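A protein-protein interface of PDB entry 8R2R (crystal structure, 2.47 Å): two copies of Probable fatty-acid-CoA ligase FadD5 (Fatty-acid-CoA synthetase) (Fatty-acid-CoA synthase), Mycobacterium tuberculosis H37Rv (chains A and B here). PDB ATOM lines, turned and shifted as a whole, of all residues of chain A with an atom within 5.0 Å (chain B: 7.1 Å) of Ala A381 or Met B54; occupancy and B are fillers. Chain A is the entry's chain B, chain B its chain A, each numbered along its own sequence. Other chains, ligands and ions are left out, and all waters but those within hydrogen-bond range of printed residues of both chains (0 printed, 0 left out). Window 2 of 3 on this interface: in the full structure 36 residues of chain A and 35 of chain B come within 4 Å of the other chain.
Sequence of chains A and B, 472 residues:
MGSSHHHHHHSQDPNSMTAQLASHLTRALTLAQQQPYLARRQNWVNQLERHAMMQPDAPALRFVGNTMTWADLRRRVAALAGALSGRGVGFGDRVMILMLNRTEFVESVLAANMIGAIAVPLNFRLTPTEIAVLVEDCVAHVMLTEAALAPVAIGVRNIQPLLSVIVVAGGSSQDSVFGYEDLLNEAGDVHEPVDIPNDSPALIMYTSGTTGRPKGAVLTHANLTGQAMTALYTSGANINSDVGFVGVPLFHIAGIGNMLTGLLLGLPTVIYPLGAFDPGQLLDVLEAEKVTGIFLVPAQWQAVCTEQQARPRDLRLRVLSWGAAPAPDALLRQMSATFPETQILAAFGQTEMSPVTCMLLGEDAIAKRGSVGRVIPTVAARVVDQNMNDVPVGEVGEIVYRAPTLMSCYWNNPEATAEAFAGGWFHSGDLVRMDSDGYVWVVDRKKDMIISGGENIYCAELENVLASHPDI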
ATOM      1  N   VAL A 375     -20.053  22.056 -12.626  1.00  0.00           N
ATOM      2  CA  VAL A 375     -21.329  22.237 -13.308  1.00  0.00           C
ATOM      3  C   VAL A 375     -22.430  22.395 -12.270  1.00  0.00           C
ATOM      4  O   VAL A 375     -22.568  21.570 -11.359  1.00  0.00           O
ATOM      5  CB  VAL A 375     -21.619  21.054 -14.243  1.00  0.00           C
ATOM      6  CG1 VAL A 375     -22.956  21.237 -14.914  1.00  0.00           C
ATOM      7  CG2 VAL A 375     -20.515  20.893 -15.271  1.00  0.00           C
ATOM      8  N   VAL A 379     -27.981  21.807 -14.150  1.00  0.00           N
ATOM      9  CA  VAL A 379     -27.477  21.630 -15.509  1.00  0.00           C
ATOM     10  C   VAL A 379     -26.803  20.265 -15.600  1.00  0.00           C
ATOM     11  O   VAL A 379     -26.041  19.886 -14.704  1.00  0.00           O
ATOM     12  CB  VAL A 379     -26.488  22.753 -15.894  1.00  0.00           C
ATOM     13  CG1 VAL A 379     -25.678  22.386 -17.120  1.00  0.00           C
ATOM     14  CG2 VAL A 379     -27.223  24.058 -16.118  1.00  0.00           C
ATOM     15  N   ALA A 380     -27.089  19.526 -16.669  1.00  0.00           N
ATOM     16  CA  ALA A 380     -26.386  18.287 -16.976  1.00  0.00           C
ATOM     17  C   ALA A 380     -25.382  18.540 -18.091  1.00  0.00           C
ATOM     18  O   ALA A 380     -25.676  19.262 -19.048  1.00  0.00           O
ATOM     19  CB  ALA A 380     -27.362  17.188 -17.395  1.00  0.00           C
ATOM     20  N   ALA A 381     -24.197  17.943 -17.970  1.00  0.00           N
ATOM     21  CA  ALA A 381     -23.148  18.160 -18.952  1.00  0.00           C
ATOM     22  C   ALA A 381     -22.399  16.865 -19.227  1.00  0.00           C
ATOM     23  O   ALA A 381     -22.223  16.025 -18.342  1.00  0.00           O
ATOM     24  CB  ALA A 381     -22.160  19.247 -18.499  1.00  0.00           C
ATOM     25  N   ARG A 382     -21.962  16.716 -20.476  1.00  0.00           N
ATOM     26  CA  ARG A 382     -21.075  15.645 -20.898  1.00  0.00           C
ATOM     27  C   ARG A 382     -19.860  16.255 -21.584  1.00  0.00           C
ATOM     28  O   ARG A 382     -19.924  17.370 -22.105  1.00  0.00           O
ATOM     29  CB  ARG A 382     -21.768  14.684 -21.868  1.00  0.00           C
ATOM     30  CG  ARG A 382     -22.990  13.971 -21.323  1.00  0.00           C
ATOM     31  CD  ARG A 382     -23.701  13.212 -22.441  1.00  0.00           C
ATOM     32  NE  ARG A 382     -22.809  12.327 -23.177  1.00  0.00           N
ATOM     33  CZ  ARG A 382     -23.058  11.865 -24.395  1.00  0.00           C
ATOM     34  NH1 ARG A 382     -24.160  12.195 -25.047  1.00  0.00           N
ATOM     35  NH2 ARG A 382     -22.174  11.061 -24.977  1.00  0.00           N
ATOM     36  N   VAL A 383     -18.753  15.515 -21.585  1.00  0.00           N
ATOM     37  CA  VAL A 383     -17.555  15.877 -22.338  1.00  0.00           C
ATOM     38  C   VAL A 383     -17.390  14.846 -23.445  1.00  0.00           C
ATOM     39  O   VAL A 383     -16.992  13.704 -23.185  1.00  0.00           O
ATOM     40  CB  VAL A 383     -16.308  15.935 -21.449  1.00  0.00           C
ATOM     41  CG1 VAL A 383     -15.130  16.454 -22.243  1.00  0.00           C
ATOM     42  CG2 VAL A 383     -16.560  16.800 -20.221  1.00  0.00           C
ATOM     43  N   ILE A 399     -17.646  20.191 -24.187  1.00  0.00           N
ATOM     44  CA  ILE A 399     -18.668  20.083 -23.154  1.00  0.00           C
ATOM     45  C   ILE A 399     -20.012  20.439 -23.770  1.00  0.00           C
ATOM     46  O   ILE A 399     -20.147  21.466 -24.450  1.00  0.00           O
ATOM     47  CB  ILE A 399     -18.341  20.975 -21.941  1.00  0.00           C
ATOM     48  CG1 ILE A 399     -19.365  20.769 -20.820  1.00  0.00           C
ATOM     49  CG2 ILE A 399     -18.258  22.443 -22.322  1.00  0.00           C
ATOM     50  CD1 ILE A 399     -18.949  21.407 -19.513  1.00  0.00           C
ATOM     51  N   VAL A 400     -20.995  19.568 -23.564  1.00  0.00           N
ATOM     52  CA  VAL A 400     -22.321  19.708 -24.144  1.00  0.00           C
ATOM     53  C   VAL A 400     -23.343  19.599 -23.023  1.00  0.00           C
ATOM     54  O   VAL A 400     -23.132  18.884 -22.039  1.00  0.00           O
ATOM     55  CB  VAL A 400     -22.559  18.649 -25.241  1.00  0.00           C
ATOM     56  CG1 VAL A 400     -21.451  18.729 -26.281  1.00  0.00           C
ATOM     57  CG2 VAL A 400     -22.608  17.258 -24.637  1.00  0.00           C
ATOM     58  N   TYR A 401     -24.450  20.325 -23.162  1.00  0.00           N
ATOM     59  CA  TYR A 401     -25.373  20.536 -22.057  1.00  0.00           C
ATOM     60  C   TYR A 401     -26.792  20.083 -22.390  1.00  0.00           C
ATOM     61  O   TYR A 401     -27.218  20.090 -23.547  1.00  0.00           O
ATOM     62  CB  TYR A 401     -25.425  22.010 -21.652  1.00  0.00           C
ATOM     63  CG  TYR A 401     -24.097  22.662 -21.318  1.00  0.00           C
ATOM     64  CD1 TYR A 401     -23.445  22.395 -20.119  1.00  0.00           C
ATOM     65  CD2 TYR A 401     -23.525  23.591 -22.181  1.00  0.00           C
ATOM     66  CE1 TYR A 401     -22.240  23.012 -19.807  1.00  0.00           C
ATOM     67  CE2 TYR A 401     -22.329  24.215 -21.876  1.00  0.00           C
ATOM     68  CZ  TYR A 401     -21.693  23.927 -20.686  1.00  0.00           C
ATOM     69  OH  TYR A 401     -20.505  24.553 -20.385  1.00  0.00           O
ATOM     70  N   TRP A 425     -27.903  17.219 -27.454  1.00  0.00           N
ATOM     71  CA  TRP A 425     -27.169  17.978 -26.450  1.00  0.00           C
ATOM     72  C   TRP A 425     -26.690  19.276 -27.078  1.00  0.00           C
ATOM     73  O   TRP A 425     -26.307  19.292 -28.251  1.00  0.00           O
ATOM     74  CB  TRP A 425     -25.970  17.182 -25.898  1.00  0.00           C
ATOM     75  CG  TRP A 425     -26.352  15.976 -25.085  1.00  0.00           C
ATOM     76  CD1 TRP A 425     -26.781  14.771 -25.556  1.00  0.00           C
ATOM     77  CD2 TRP A 425     -26.329  15.861 -23.656  1.00  0.00           C
ATOM     78  NE1 TRP A 425     -27.033  13.914 -24.509  1.00  0.00           N
ATOM     79  CE2 TRP A 425     -26.769  14.563 -23.333  1.00  0.00           C
ATOM     80  CE3 TRP A 425     -25.983  16.732 -22.618  1.00  0.00           C
ATOM     81  CZ2 TRP A 425     -26.878  14.118 -22.019  1.00  0.00           C
ATOM     82  CZ3 TRP A 425     -26.095  16.289 -21.315  1.00  0.00           C
ATOM     83  CH2 TRP A 425     -26.531  14.991 -21.025  1.00  0.00           C
ATOM     84  N   MET A 434     -12.837  17.594 -17.487  1.00  0.00           N
ATOM     85  CA  MET A 434     -13.350  17.445 -16.134  1.00  0.00           C
ATOM     86  C   MET A 434     -12.465  16.475 -15.360  1.00  0.00           C
ATOM     87  O   MET A 434     -11.971  15.492 -15.917  1.00  0.00           O
ATOM     88  CB  MET A 434     -14.796  16.953 -16.159  1.00  0.00           C
ATOM     89  CG  MET A 434     -15.739  17.775 -15.308  1.00  0.00           C
ATOM     90  SD  MET A 434     -17.451  17.294 -15.564  1.00  0.00           S
ATOM     91  CE  MET A 434     -17.428  15.621 -14.921  1.00  0.00           C
ATOM     92  N   LEU B  48     -33.086  14.011  -9.843  1.00  0.00           N
ATOM     93  CA  LEU B  48     -32.456  12.782  -9.378  1.00  0.00           C
ATOM     94  C   LEU B  48     -31.669  12.106 -10.495  1.00  0.00           C
ATOM     95  O   LEU B  48     -30.548  11.631 -10.275  1.00  0.00           O
ATOM     96  CB  LEU B  48     -33.516  11.838  -8.810  1.00  0.00           C
ATOM     97  CG  LEU B  48     -33.062  10.403  -8.537  1.00  0.00           C
ATOM     98  CD1 LEU B  48     -32.058  10.354  -7.387  1.00  0.00           C
ATOM     99  CD2 LEU B  48     -34.262   9.497  -8.268  1.00  0.00           C
ATOM    100  N   GLU B  49     -32.233  12.054 -11.703  1.00  0.00           N
ATOM    101  CA  GLU B  49     -31.485  11.501 -12.828  1.00  0.00           C
ATOM    102  C   GLU B  49     -30.257  12.353 -13.139  1.00  0.00           C
ATOM    103  O   GLU B  49     -29.172  11.818 -13.400  1.00  0.00           O
ATOM    104  CB  GLU B  49     -32.388  11.377 -14.055  1.00  0.00           C
ATOM    105  CG  GLU B  49     -33.728  10.690 -13.802  1.00  0.00           C
ATOM    106  CD  GLU B  49     -33.740   9.220 -14.190  1.00  0.00           C
ATOM    107  OE1 GLU B  49     -32.669   8.579 -14.135  1.00  0.00           O
ATOM    108  OE2 GLU B  49     -34.820   8.706 -14.555  1.00  0.00           O
ATOM    109  N   ARG B  50     -30.403  13.681 -13.090  1.00  0.00           N
ATOM    110  CA  ARG B  50     -29.262  14.567 -13.319  1.00  0.00           C
ATOM    111  C   ARG B  50     -28.160  14.324 -12.299  1.00  0.00           C
ATOM    112  O   ARG B  50     -26.975  14.290 -12.652  1.00  0.00           O
ATOM    113  CB  ARG B  50     -29.713  16.033 -13.284  1.00  0.00           C
ATOM    114  CG  ARG B  50     -28.794  17.000 -12.492  1.00  0.00           C
ATOM    115  CD  ARG B  50     -27.570  17.344 -13.293  1.00  0.00           C
ATOM    116  NE  ARG B  50     -26.709  18.384 -12.739  1.00  0.00           N
ATOM    117  CZ  ARG B  50     -25.885  18.241 -11.709  1.00  0.00           C
ATOM    118  NH1 ARG B  50     -25.961  17.205 -10.895  1.00  0.00           N
ATOM    119  NH2 ARG B  50     -24.951  19.164 -11.496  1.00  0.00           N
ATOM    120  N   HIS B  51     -28.527  14.169 -11.023  1.00  0.00           N
ATOM    121  CA  HIS B  51     -27.515  13.993  -9.986  1.00  0.00           C
ATOM    122  C   HIS B  51     -26.855  12.626 -10.091  1.00  0.00           C
ATOM    123  O   HIS B  51     -25.645  12.497  -9.874  1.00  0.00           O
ATOM    124  CB  HIS B  51     -28.131  14.185  -8.602  1.00  0.00           C
ATOM    125  CG  HIS B  51     -28.696  15.547  -8.376  1.00  0.00           C
ATOM    126  ND1 HIS B  51     -28.056  16.694  -8.790  1.00  0.00           N
ATOM    127  CD2 HIS B  51     -29.845  15.947  -7.780  1.00  0.00           C
ATOM    128  CE1 HIS B  51     -28.787  17.744  -8.461  1.00  0.00           C
ATOM    129  NE2 HIS B  51     -29.877  17.318  -7.846  1.00  0.00           N
ATOM    130  N   ALA B  52     -27.633  11.591 -10.417  1.00  0.00           N
ATOM    131  CA  ALA B  52     -27.052  10.266 -10.590  1.00  0.00           C
ATOM    132  C   ALA B  52     -26.034  10.238 -11.722  1.00  0.00           C
ATOM    133  O   ALA B  52     -25.125   9.404 -11.702  1.00  0.00           O
ATOM    134  CB  ALA B  52     -28.151   9.230 -10.837  1.00  0.00           C
ATOM    135  N   MET B  53     -26.147  11.147 -12.691  1.00  0.00           N
ATOM    136  CA  MET B  53     -25.183  11.205 -13.782  1.00  0.00           C
ATOM    137  C   MET B  53     -23.972  12.072 -13.460  1.00  0.00           C
ATOM    138  O   MET B  53     -22.841  11.696 -13.782  1.00  0.00           O
ATOM    139  CB  MET B  53     -25.852  11.724 -15.053  1.00  0.00           C
ATOM    140  CG  MET B  53     -24.871  12.368 -16.010  1.00  0.00           C
ATOM    141  SD  MET B  53     -25.626  12.821 -17.568  1.00  0.00           S
ATOM    142  CE  MET B  53     -27.117  13.607 -16.968  1.00  0.00           C
ATOM    143  N   MET B  54     -24.174  13.229 -12.831  1.00  0.00           N
ATOM    144  CA  MET B  54     -23.064  14.145 -12.603  1.00  0.00           C
ATOM    145  C   MET B  54     -22.275  13.829 -11.340  1.00  0.00           C
ATOM    146  O   MET B  54     -21.075  14.118 -11.279  1.00  0.00           O
ATOM    147  CB  MET B  54     -23.582  15.582 -12.545  1.00  0.00           C
ATOM    148  CG  MET B  54     -24.416  15.963 -13.750  1.00  0.00           C
ATOM    149  SD  MET B  54     -23.486  15.856 -15.283  1.00  0.00           S
ATOM    150  CE  MET B  54     -22.333  17.209 -15.047  1.00  0.00           C
ATOM    151  N   GLN B  55     -22.907  13.249 -10.344  1.00  0.00           N
ATOM    152  CA  GLN B  55     -22.204  12.941  -9.109  1.00  0.00           C
ATOM    153  C   GLN B  55     -22.750  11.650  -8.511  1.00  0.00           C
ATOM    154  O   GLN B  55     -23.280  11.675  -7.394  1.00  0.00           O
ATOM    155  CB  GLN B  55     -22.342  14.100  -8.115  1.00  0.00           C
ATOM    156  CG  GLN B  55     -23.732  14.713  -8.064  1.00  0.00           C
ATOM    157  CD  GLN B  55     -23.895  15.698  -6.920  1.00  0.00           C
ATOM    158  OE1 GLN B  55     -22.918  16.167  -6.337  1.00  0.00           O
ATOM    159  NE2 GLN B  55     -25.140  16.008  -6.590  1.00  0.00           N
ATOM    160  N   PRO B  56     -22.639  10.509  -9.210  1.00  0.00           N
ATOM    161  CA  PRO B  56     -23.326   9.294  -8.731  1.00  0.00           C
ATOM    162  C   PRO B  56     -22.937   8.889  -7.325  1.00  0.00           C
ATOM    163  O   PRO B  56     -23.798   8.425  -6.568  1.00  0.00           O
ATOM    164  CB  PRO B  56     -22.913   8.233  -9.762  1.00  0.00           C
ATOM    165  CG  PRO B  56     -21.646   8.744 -10.329  1.00  0.00           C
ATOM    166  CD  PRO B  56     -21.822  10.229 -10.401  1.00  0.00           C
ATOM    167  N   ASP B  57     -21.676   9.085  -6.939  1.00  0.00           N
ATOM    168  CA  ASP B  57     -21.178   8.609  -5.657  1.00  0.00           C
ATOM    169  C   ASP B  57     -21.224   9.674  -4.570  1.00  0.00           C
ATOM    170  O   ASP B  57     -20.663   9.464  -3.490  1.00  0.00           O
ATOM    171  CB  ASP B  57     -19.756   8.074  -5.814  1.00  0.00           C
ATOM    172  CG  ASP B  57     -19.666   6.963  -6.840  1.00  0.00           C
ATOM    173  OD1 ASP B  57     -20.665   6.226  -6.996  1.00  0.00           O
ATOM    174  OD2 ASP B  57     -18.607   6.830  -7.497  1.00  0.00           O
ATOM    175  N   ALA B  58     -21.894  10.794  -4.819  1.00  0.00           N
ATOM    176  CA  ALA B  58     -22.078  11.825  -3.811  1.00  0.00           C
ATOM    177  C   ALA B  58     -23.240  11.466  -2.887  1.00  0.00           C
ATOM    178  O   ALA B  58     -24.183  10.787  -3.299  1.00  0.00           O
ATOM    179  CB  ALA B  58     -22.341  13.173  -4.474  1.00  0.00           C
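NH2 of Arg B50 lies within hydrogen-bond range of O of Val A375 (3.4 Å).
NE of Arg B50 lies within hydrogen-bond range of O of Val A379 (2.6 Å).
The side-chain sulfur (SD) of Met B54 lies within hydrogen-bond range of the backbone NH (N) of Ala A381, at 3.5 Å.
ND1 of His B51 sits at hydrogen-bond distance from NH1 of Arg B50, at 3.0 Å.
Among the printed residues, pairs that only touch across the chains: Ala A380 with Met B53 (3.6 Å), Ala A380 with Arg B50 (3.98 Å) and Val A375 with Met B54 (3.99 Å).
Of the printed residues of chain B, Val A379 touches Arg B50.
Of chain B, only Met B54 comes within 4 Å of Ala A381.
Ile A399 touches none of the printed residues of chain B.
Trp A425 touches none of the printed residues of chain B.
Of the printed residues of chain A, Arg B50 touches Val A375 (3.4 Å), Val A379 (2.6 Å) and Ala A380 (3.98 Å).
Of the printed residues of chain A, Met B53 touches Ala A380 (3.6 Å).
The nearest printed residue of chain B that does not touch Val A379 is Met B54 (4.4 Å).
Printed residues of chain A that touch a printed residue of chain B: Val A375, Val A379, Ala A380 and Ala A381.
Hydrophobic or aromatic side chains of chain A within 4 Å of the printed part of chain B: Val A375 and Ala A380.
No position is printed for both chains.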
